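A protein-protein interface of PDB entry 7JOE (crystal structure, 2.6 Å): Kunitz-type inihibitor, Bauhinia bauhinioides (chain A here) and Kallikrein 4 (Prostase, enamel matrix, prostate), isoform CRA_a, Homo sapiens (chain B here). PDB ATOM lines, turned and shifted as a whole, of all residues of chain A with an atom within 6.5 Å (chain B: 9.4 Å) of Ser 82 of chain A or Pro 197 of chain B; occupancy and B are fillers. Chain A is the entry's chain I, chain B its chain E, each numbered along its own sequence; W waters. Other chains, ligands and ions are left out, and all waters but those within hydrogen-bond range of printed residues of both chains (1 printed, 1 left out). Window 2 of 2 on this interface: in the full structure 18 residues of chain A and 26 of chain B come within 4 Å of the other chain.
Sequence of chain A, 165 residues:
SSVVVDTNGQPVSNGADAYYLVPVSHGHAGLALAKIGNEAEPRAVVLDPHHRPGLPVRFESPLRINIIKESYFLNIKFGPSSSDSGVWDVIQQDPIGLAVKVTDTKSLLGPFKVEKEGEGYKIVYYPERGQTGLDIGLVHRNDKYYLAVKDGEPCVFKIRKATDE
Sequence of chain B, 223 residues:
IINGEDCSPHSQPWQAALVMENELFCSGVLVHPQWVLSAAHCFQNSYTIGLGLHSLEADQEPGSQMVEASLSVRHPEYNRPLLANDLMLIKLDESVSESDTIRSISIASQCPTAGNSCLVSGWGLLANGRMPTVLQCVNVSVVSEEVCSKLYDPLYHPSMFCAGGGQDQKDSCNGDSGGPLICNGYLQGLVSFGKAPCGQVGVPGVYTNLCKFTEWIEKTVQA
The side-chain carboxylate (OD2) of Asp 171 of chain B is in salt-bridge range of the guanidinium group (NH2) of Arg 64 of chain A (3.3 Å). The guanidinium group (NE) of Arg 64 of chain A lies within hydrogen-bond range of the backbone carbonyl oxygen (O) of Ser 172 of chain B, at 3.1 Å. The side-chain sulfur (SG) of Cys 198 of chain B lies close to the guanidinium group (NH1) of Arg 64 of chain A, at 3.5 Å. The backbone carbonyl oxygen (O) of Ala 196 of chain B lies within hydrogen-bond range of the side-chain amino group (NZ) of Lys 106 of chain A (3.1 Å). The backbone carbonyl oxygen of Gly 194 of chain B lies within hydrogen-bond range of the guanidinium group of Arg 64 of chain A (3.4 Å). The guanidinium group of Arg 64 of chain A lies within hydrogen-bond range of the backbone carbonyl oxygen of Lys 195 of chain B (3.1 Å).
The side-chain carboxylate (OE2) of Glu 60 of chain A lies within salt-bridge range of the side-chain amino group (NZ) of Lys 77 of chain A (2.7 Å). The backbone NH (N) of Ile 2 of chain B lies within hydrogen-bond range of the backbone carbonyl oxygen (O) of Asp 171 of chain B (2.7 Å). O of Ser 172 of chain B lies within hydrogen-bond range of SG of Cys 198 of chain B (3.4 Å). OH of Tyr 152 of chain B sits at hydrogen-bond distance from N of Lys 195 of chain B (3.3 Å). OD2 of Asp 171 of chain B is in hydrogen-bond range of N of Gly 199 of chain B, 3.4 Å away. The side-chain carboxylate (OD1) of Asp 84 of chain A is in salt-bridge range of the side-chain amino group (NZ) of Lys 106 of chain A (3.1 Å).
Among the printed residues, pairs that only touch across the chains: Glu 60 of chain A with Ala 196 of chain B (3.8 Å), Arg 64 of chain A with Cys 173 of chain B (3.6 Å), Arg 64 of chain A with Asn 174 of chain B (3.8 Å), Arg 64 of chain A with Phe 193 of chain B (3.96 Å) and Ser 82 of chain A with Pro 197 of chain B (3.9 Å).
Of the printed residues of chain B, Arg 64 of chain A touches Asp 171 (3.3 Å), Ser 172 (3.1 Å), Cys 173 (3.6 Å), Asn 174 (3.8 Å), Phe 193 (3.96 Å), Gly 194 (3.4 Å), Lys 195 (3.1 Å) and Cys 198 (3.3 Å). Ser 81 of chain A touches none of the printed residues of chain B. Of the printed residues of chain B, Ser 82 of chain A touches Pro 197. No residue of chain B comes within 4 Å of Ser 83 of chain A. Asp 84 of chain A touches none of the printed residues of chain B. Tyr 152 of chain B touches none of the printed residues of chain A. Of the printed residues of chain A, Cys 173 of chain B touches Arg 64 (3.6 Å). Pro 197 of chain B touches just one residue of chain A: Ser 82 (3.9 Å). The nearest residue of chain B that does not touch Ser 82 of chain A is Ala 196 of chain B (5.6 Å). The nearest residue of chain A that does not touch Pro 197 of chain B is Ser 81 of chain A (4.2 Å).
Of the 9 printed residues of chain A, 4 touch a printed residue of chain B. Printed residues of chain A that touch a printed residue of chain B: Glu 60, Arg 64, Ser 82 and Lys 106. Hydrophobic or aromatic side chains of chain B that line the printed part of chain A: Ala 196 and Pro 197. Among the printed residues, Asp or Glu carboxylates within 4 Å of a Lys or Arg side-chain nitrogen of the other chain: Arg 64 of chain A with Asp 171 of chain B.
Water W1 lies within hydrogen-bond range of NE of Arg 64 of chain A (2.7 Å), OD1 of Asp 171 of chain B (2.8 Å) and O of Ser 172 of chain B (3.0 Å).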
ATOM      1  N   GLU A  60      17.849 -15.918 -16.591  1.00  0.00           N
ATOM      2  CA  GLU A  60      18.008 -14.471 -16.444  1.00  0.00           C
ATOM      3  C   GLU A  60      19.468 -14.120 -16.472  1.00  0.00           C
ATOM      4  O   GLU A  60      20.208 -14.764 -15.686  1.00  0.00           O
ATOM      5  CB  GLU A  60      17.691 -14.004 -15.049  1.00  0.00           C
ATOM      6  CG  GLU A  60      16.256 -13.618 -14.833  1.00  0.00           C
ATOM      7  CD  GLU A  60      16.028 -13.102 -13.419  1.00  0.00           C
ATOM      8  OE1 GLU A  60      17.050 -13.059 -12.592  1.00  0.00           O
ATOM      9  OE2 GLU A  60      14.838 -12.782 -13.154  1.00  0.00           O
ATOM     10  N   ARG A  64      21.060  -6.227 -20.489  1.00  0.00           N
ATOM     11  CA  ARG A  64      19.757  -5.735 -20.960  1.00  0.00           C
ATOM     12  C   ARG A  64      19.545  -6.228 -22.375  1.00  0.00           C
ATOM     13  O   ARG A  64      19.145  -5.457 -23.205  1.00  0.00           O
ATOM     14  CB  ARG A  64      19.733  -4.217 -20.822  1.00  0.00           C
ATOM     15  CG  ARG A  64      19.601  -3.806 -19.371  1.00  0.00           C
ATOM     16  CD  ARG A  64      18.294  -4.348 -18.862  1.00  0.00           C
ATOM     17  NE  ARG A  64      17.968  -3.629 -17.648  1.00  0.00           N
ATOM     18  CZ  ARG A  64      17.812  -4.191 -16.463  1.00  0.00           C
ATOM     19  NH1 ARG A  64      17.908  -5.508 -16.373  1.00  0.00           N
ATOM     20  NH2 ARG A  64      17.535  -3.423 -15.408  1.00  0.00           N
ATOM     21  N   LYS A  77      15.543 -20.399 -12.786  1.00  0.00           N
ATOM     22  CA  LYS A  77      14.460 -20.345 -11.784  1.00  0.00           C
ATOM     23  C   LYS A  77      13.137 -20.805 -12.404  1.00  0.00           C
ATOM     24  O   LYS A  77      12.956 -20.666 -13.665  1.00  0.00           O
ATOM     25  CB  LYS A  77      14.394 -18.951 -11.173  1.00  0.00           C
ATOM     26  CG  LYS A  77      13.564 -17.925 -11.939  1.00  0.00           C
ATOM     27  CD  LYS A  77      13.551 -16.541 -11.261  1.00  0.00           C
ATOM     28  CE  LYS A  77      12.742 -15.488 -11.994  1.00  0.00           C
ATOM     29  NZ  LYS A  77      13.123 -14.125 -11.538  1.00  0.00           N
ATOM     30  N   PRO A  80       6.995 -17.425 -12.390  1.00  0.00           N
ATOM     31  CA  PRO A  80       7.038 -16.240 -13.232  1.00  0.00           C
ATOM     32  C   PRO A  80       8.244 -15.351 -12.899  1.00  0.00           C
ATOM     33  O   PRO A  80       8.853 -15.558 -11.843  1.00  0.00           O
ATOM     34  CB  PRO A  80       5.738 -15.509 -12.876  1.00  0.00           C
ATOM     35  CG  PRO A  80       5.555 -15.843 -11.426  1.00  0.00           C
ATOM     36  CD  PRO A  80       5.968 -17.299 -11.338  1.00  0.00           C
ATOM     37  N   SER A  81       8.486 -14.374 -13.790  1.00  0.00           N
ATOM     38  CA  SER A  81       9.597 -13.382 -13.804  1.00  0.00           C
ATOM     39  C   SER A  81       9.683 -12.622 -12.483  1.00  0.00           C
ATOM     40  O   SER A  81      10.743 -12.665 -11.857  1.00  0.00           O
ATOM     41  CB  SER A  81       9.425 -12.412 -14.939  1.00  0.00           C
ATOM     42  OG  SER A  81      10.257 -12.757 -16.036  1.00  0.00           O
ATOM     43  N   SER A  82       8.626 -11.901 -12.095  1.00  0.00           N
ATOM     44  CA  SER A  82       8.612 -11.114 -10.830  1.00  0.00           C
ATOM     45  C   SER A  82       9.321 -11.953  -9.752  1.00  0.00           C
ATOM     46  O   SER A  82      10.393 -11.490  -9.267  1.00  0.00           O
ATOM     47  CB  SER A  82       7.218 -10.718 -10.422  1.00  0.00           C
ATOM     48  OG  SER A  82       6.377 -11.860 -10.436  1.00  0.00           O
ATOM     49  N   SER A  83       8.815 -13.185  -9.545  1.00  0.00           N
ATOM     50  CA  SER A  83       9.095 -14.133  -8.433  1.00  0.00           C
ATOM     51  C   SER A  83      10.561 -14.593  -8.367  1.00  0.00           C
ATOM     52  O   SER A  83      11.105 -14.971  -9.423  1.00  0.00           O
ATOM     53  CB  SER A  83       8.206 -15.329  -8.561  1.00  0.00           C
ATOM     54  OG  SER A  83       8.447 -16.214  -7.481  1.00  0.00           O
ATOM     55  N   ASP A  84      11.115 -14.677  -7.144  1.00  0.00           N
ATOM     56  CA  ASP A  84      12.485 -15.179  -6.829  1.00  0.00           C
ATOM     57  C   ASP A  84      12.420 -16.372  -5.861  1.00  0.00           C
ATOM     58  O   ASP A  84      13.431 -16.639  -5.158  1.00  0.00           O
ATOM     59  CB  ASP A  84      13.330 -14.070  -6.197  1.00  0.00           C
ATOM     60  CG  ASP A  84      13.801 -13.019  -7.184  1.00  0.00           C
ATOM     61  OD1 ASP A  84      13.389 -13.098  -8.361  1.00  0.00           O
ATOM     62  OD2 ASP A  84      14.590 -12.140  -6.766  1.00  0.00           O
ATOM     63  N   LYS A 106      18.522 -14.577  -4.344  1.00  0.00           N
ATOM     64  CA  LYS A 106      19.179 -14.426  -5.681  1.00  0.00           C
ATOM     65  C   LYS A 106      20.398 -13.486  -5.660  1.00  0.00           C
ATOM     66  O   LYS A 106      20.283 -12.399  -5.132  1.00  0.00           O
ATOM     67  CB  LYS A 106      18.147 -13.862  -6.654  1.00  0.00           C
ATOM     68  CG  LYS A 106      18.710 -13.592  -8.026  1.00  0.00           C
ATOM     69  CD  LYS A 106      17.683 -13.630  -9.109  1.00  0.00           C
ATOM     70  CE  LYS A 106      17.206 -12.262  -9.521  1.00  0.00           C
ATOM     71  NZ  LYS A 106      15.852 -12.401 -10.083  1.00  0.00           N
ATOM     72  N   ILE B   2      11.268   1.377 -20.044  1.00  0.00           N
ATOM     73  CA  ILE B   2      10.155   1.278 -19.064  1.00  0.00           C
ATOM     74  C   ILE B   2       9.625   2.686 -18.793  1.00  0.00           C
ATOM     75  O   ILE B   2      10.383   3.466 -18.245  1.00  0.00           O
ATOM     76  CB  ILE B   2      10.698   0.612 -17.781  1.00  0.00           C
ATOM     77  CG1 ILE B   2      11.044  -0.863 -18.006  1.00  0.00           C
ATOM     78  CG2 ILE B   2       9.796   0.831 -16.559  1.00  0.00           C
ATOM     79  CD1 ILE B   2       9.952  -1.672 -18.627  1.00  0.00           C
ATOM     80  N   ALA B 127       6.852  -1.471 -19.969  1.00  0.00           N
ATOM     81  CA  ALA B 127       6.347  -1.815 -18.605  1.00  0.00           C
ATOM     82  C   ALA B 127       5.491  -3.111 -18.623  1.00  0.00           C
ATOM     83  O   ALA B 127       5.544  -3.868 -17.647  1.00  0.00           O
ATOM     84  CB  ALA B 127       5.601  -0.604 -18.034  1.00  0.00           C
ATOM     85  N   TYR B 152      25.306  -2.467  -6.001  1.00  0.00           N
ATOM     86  CA  TYR B 152      25.903  -3.352  -7.033  1.00  0.00           C
ATOM     87  C   TYR B 152      27.261  -3.901  -6.624  1.00  0.00           C
ATOM     88  O   TYR B 152      27.815  -4.561  -7.532  1.00  0.00           O
ATOM     89  CB  TYR B 152      26.090  -2.617  -8.356  1.00  0.00           C
ATOM     90  CG  TYR B 152      24.789  -2.490  -9.111  1.00  0.00           C
ATOM     91  CD1 TYR B 152      24.176  -3.585  -9.725  1.00  0.00           C
ATOM     92  CD2 TYR B 152      24.132  -1.280  -9.190  1.00  0.00           C
ATOM     93  CE1 TYR B 152      22.974  -3.478 -10.417  1.00  0.00           C
ATOM     94  CE2 TYR B 152      22.916  -1.153  -9.846  1.00  0.00           C
ATOM     95  CZ  TYR B 152      22.352  -2.241 -10.481  1.00  0.00           C
ATOM     96  OH  TYR B 152      21.147  -2.098 -11.076  1.00  0.00           O
ATOM     97  N   GLN B 169       9.793   5.341 -11.726  1.00  0.00           N
ATOM     98  CA  GLN B 169      10.146   3.971 -12.181  1.00  0.00           C
ATOM     99  C   GLN B 169      10.470   3.968 -13.673  1.00  0.00           C
ATOM    100  O   GLN B 169       9.903   3.160 -14.431  1.00  0.00           O
ATOM    101  CB  GLN B 169       9.017   2.978 -11.936  1.00  0.00           C
ATOM    102  CG  GLN B 169       8.863   2.573 -10.489  1.00  0.00           C
ATOM    103  CD  GLN B 169       8.049   1.307 -10.426  1.00  0.00           C
ATOM    104  OE1 GLN B 169       7.027   1.157 -11.096  1.00  0.00           O
ATOM    105  NE2 GLN B 169       8.517   0.363  -9.635  1.00  0.00           N
ATOM    106  N   ASP B 171      13.462   3.301 -16.531  1.00  0.00           N
ATOM    107  CA  ASP B 171      14.613   2.388 -16.669  1.00  0.00           C
ATOM    108  C   ASP B 171      14.686   1.833 -18.094  1.00  0.00           C
ATOM    109  O   ASP B 171      13.697   1.873 -18.865  1.00  0.00           O
ATOM    110  CB  ASP B 171      14.552   1.269 -15.605  1.00  0.00           C
ATOM    111  CG  ASP B 171      15.824   0.426 -15.417  1.00  0.00           C
ATOM    112  OD1 ASP B 171      16.928   0.907 -15.873  1.00  0.00           O
ATOM    113  OD2 ASP B 171      15.722  -0.729 -14.837  1.00  0.00           O
ATOM    114  N   SER B 172      15.860   1.264 -18.357  1.00  0.00           N
ATOM    115  CA  SER B 172      16.179   0.393 -19.505  1.00  0.00           C
ATOM    116  C   SER B 172      15.681  -1.030 -19.269  1.00  0.00           C
ATOM    117  O   SER B 172      15.797  -1.528 -18.114  1.00  0.00           O
ATOM    118  CB  SER B 172      17.634   0.429 -19.753  1.00  0.00           C
ATOM    119  OG  SER B 172      17.921   1.659 -20.404  1.00  0.00           O
ATOM    120  N   CYS B 173      15.179  -1.659 -20.335  1.00  0.00           N
ATOM    121  CA  CYS B 173      14.729  -3.061 -20.291  1.00  0.00           C
ATOM    122  C   CYS B 173      15.396  -3.931 -21.351  1.00  0.00           C
ATOM    123  O   CYS B 173      16.401  -3.496 -21.994  1.00  0.00           O
ATOM    124  CB  CYS B 173      13.222  -3.172 -20.391  1.00  0.00           C
ATOM    125  SG  CYS B 173      12.678  -4.591 -19.400  1.00  0.00           S
ATOM    126  N   ASN B 174      14.871  -5.140 -21.496  1.00  0.00           N
ATOM    127  CA  ASN B 174      15.551  -6.165 -22.316  1.00  0.00           C
ATOM    128  C   ASN B 174      15.393  -5.815 -23.798  1.00  0.00           C
ATOM    129  O   ASN B 174      14.263  -5.650 -24.231  1.00  0.00           O
ATOM    130  CB  ASN B 174      15.042  -7.558 -21.963  1.00  0.00           C
ATOM    131  CG  ASN B 174      15.622  -8.115 -20.679  1.00  0.00           C
ATOM    132  OD1 ASN B 174      16.278  -7.435 -19.897  1.00  0.00           O
ATOM    133  ND2 ASN B 174      15.419  -9.389 -20.472  1.00  0.00           N
ATOM    134  N   PHE B 193      23.413  -3.180 -17.870  1.00  0.00           N
ATOM    135  CA  PHE B 193      22.742  -4.173 -16.993  1.00  0.00           C
ATOM    136  C   PHE B 193      22.003  -3.449 -15.886  1.00  0.00           C
ATOM    137  O   PHE B 193      21.979  -2.241 -15.846  1.00  0.00           O
ATOM    138  CB  PHE B 193      23.715  -5.236 -16.445  1.00  0.00           C
ATOM    139  CG  PHE B 193      24.766  -4.760 -15.459  1.00  0.00           C
ATOM    140  CD1 PHE B 193      25.951  -4.182 -15.890  1.00  0.00           C
ATOM    141  CD2 PHE B 193      24.611  -4.948 -14.089  1.00  0.00           C
ATOM    142  CE1 PHE B 193      26.931  -3.805 -14.983  1.00  0.00           C
ATOM    143  CE2 PHE B 193      25.589  -4.553 -13.187  1.00  0.00           C
ATOM    144  CZ  PHE B 193      26.761  -4.019 -13.635  1.00  0.00           C
ATOM    145  N   GLY B 194      21.341  -4.240 -15.074  1.00  0.00           N
ATOM    146  CA  GLY B 194      20.647  -3.813 -13.860  1.00  0.00           C
ATOM    147  C   GLY B 194      20.064  -5.040 -13.213  1.00  0.00           C
ATOM    148  O   GLY B 194      20.064  -6.118 -13.876  1.00  0.00           O
ATOM    149  N   LYS B 195      19.522  -4.872 -12.013  1.00  0.00           N
ATOM    150  CA  LYS B 195      18.716  -5.925 -11.346  1.00  0.00           C
ATOM    151  C   LYS B 195      17.609  -6.386 -12.298  1.00  0.00           C
ATOM    152  O   LYS B 195      17.359  -5.688 -13.308  1.00  0.00           O
ATOM    153  CB  LYS B 195      18.238  -5.388  -9.998  1.00  0.00           C
ATOM    154  CG  LYS B 195      19.414  -4.927  -9.159  1.00  0.00           C
ATOM    155  CD  LYS B 195      19.125  -4.792  -7.720  1.00  0.00           C
ATOM    156  CE  LYS B 195      20.369  -4.975  -6.877  1.00  0.00           C
ATOM    157  NZ  LYS B 195      19.993  -5.310  -5.478  1.00  0.00           N
ATOM    158  N   ALA B 196      17.021  -7.557 -12.021  1.00  0.00           N
ATOM    159  CA  ALA B 196      15.999  -8.237 -12.859  1.00  0.00           C
ATOM    160  C   ALA B 196      14.922  -8.762 -11.918  1.00  0.00           C
ATOM    161  O   ALA B 196      15.276  -9.474 -10.977  1.00  0.00           O
ATOM    162  CB  ALA B 196      16.665  -9.333 -13.667  1.00  0.00           C
ATOM    163  N   PRO B 197      13.620  -8.385 -12.051  1.00  0.00           N
ATOM    164  CA  PRO B 197      13.097  -7.530 -13.128  1.00  0.00           C
ATOM    165  C   PRO B 197      13.550  -6.060 -13.288  1.00  0.00           C
ATOM    166  O   PRO B 197      13.980  -5.455 -12.323  1.00  0.00           O
ATOM    167  CB  PRO B 197      11.619  -7.327 -12.740  1.00  0.00           C
ATOM    168  CG  PRO B 197      11.276  -8.460 -11.834  1.00  0.00           C
ATOM    169  CD  PRO B 197      12.559  -8.762 -11.100  1.00  0.00           C
ATOM    170  N   CYS B 198      13.347  -5.496 -14.490  1.00  0.00           N
ATOM    171  CA  CYS B 198      13.514  -4.053 -14.812  1.00  0.00           C
ATOM    172  C   CYS B 198      12.460  -3.242 -14.090  1.00  0.00           C
ATOM    173  O   CYS B 198      11.354  -3.743 -13.946  1.00  0.00           O
ATOM    174  CB  CYS B 198      13.342  -3.771 -16.295  1.00  0.00           C
ATOM    175  SG  CYS B 198      14.602  -4.642 -17.259  1.00  0.00           S
ATOM    176  N   GLY B 199      12.811  -2.034 -13.681  1.00  0.00           N
ATOM    177  CA  GLY B 199      11.844  -1.040 -13.207  1.00  0.00           C
ATOM    178  C   GLY B 199      11.533  -1.185 -11.733  1.00  0.00           C
ATOM    179  O   GLY B 199      10.564  -0.508 -11.294  1.00  0.00           O
ATOM    180  N   GLN B 200      12.324  -1.980 -10.997  1.00  0.00           N
ATOM    181  CA  GLN B 200      12.306  -2.012  -9.506  1.00  0.00           C
ATOM    182  C   GLN B 200      12.350  -0.551  -8.982  1.00  0.00           C
ATOM    183  O   GLN B 200      13.149   0.262  -9.500  1.00  0.00           O
ATOM    184  CB  GLN B 200      13.443  -2.911  -8.990  1.00  0.00           C
ATOM    185  CG  GLN B 200      13.020  -4.294  -8.467  1.00  0.00           C
ATOM    186  CD  GLN B 200      13.983  -5.391  -8.878  1.00  0.00           C
ATOM    187  OE1 GLN B 200      14.865  -5.769  -8.133  1.00  0.00           O
ATOM    188  NE2 GLN B 200      13.836  -5.925 -10.079  1.00  0.00           N
ATOM    189  N   VAL B 201      11.465  -0.205  -8.037  1.00  0.00           N
ATOM    190  CA  VAL B 201      11.335   1.158  -7.424  1.00  0.00           C
ATOM    191  C   VAL B 201      12.669   1.496  -6.776  1.00  0.00           C
ATOM    192  O   VAL B 201      13.092   0.697  -5.918  1.00  0.00           O
ATOM    193  CB  VAL B 201      10.252   1.197  -6.331  1.00  0.00           C
ATOM    194  CG1 VAL B 201       8.858   0.929  -6.875  1.00  0.00           C
ATOM    195  CG2 VAL B 201      10.571   0.226  -5.199  1.00  0.00           C
ATOM    196  N   VAL B 203      15.661   1.548  -8.039  1.00  0.00           N
ATOM    197  CA  VAL B 203      16.770   0.707  -8.552  1.00  0.00           C
ATOM    198  C   VAL B 203      17.239   1.214  -9.935  1.00  0.00           C
ATOM    199  O   VAL B 203      16.666   0.909 -10.991  1.00  0.00           O
ATOM    200  CB  VAL B 203      16.387  -0.790  -8.529  1.00  0.00           C
ATOM    201  CG1 VAL B 203      17.471  -1.649  -9.181  1.00  0.00           C
ATOM    202  CG2 VAL B 203      16.078  -1.311  -7.108  1.00  0.00           C
ATOM    203  N   PRO B 204      18.375   1.953  -9.978  1.00  0.00           N
ATOM    204  CA  PRO B 204      18.939   2.421 -11.242  1.00  0.00           C
ATOM    205  C   PRO B 204      19.497   1.276 -12.089  1.00  0.00           C
ATOM    206  O   PRO B 204      19.814   0.243 -11.524  1.00  0.00           O
ATOM    207  CB  PRO B 204      20.129   3.330 -10.853  1.00  0.00           C
ATOM    208  CG  PRO B 204      20.527   2.846  -9.475  1.00  0.00           C
ATOM    209  CD  PRO B 204      19.228   2.361  -8.842  1.00  0.00           C
ATOM    210  N   GLY B 205      19.600   1.526 -13.388  1.00  0.00           N
ATOM    211  CA  GLY B 205      20.350   0.672 -14.330  1.00  0.00           C
ATOM    212  C   GLY B 205      21.791   1.093 -14.350  1.00  0.00           C
ATOM    213  O   GLY B 205      22.044   2.177 -13.945  1.00  0.00           O
HETATM  214  O   HOH W   1      18.537  -1.022 -16.997  1.00  0.00           O
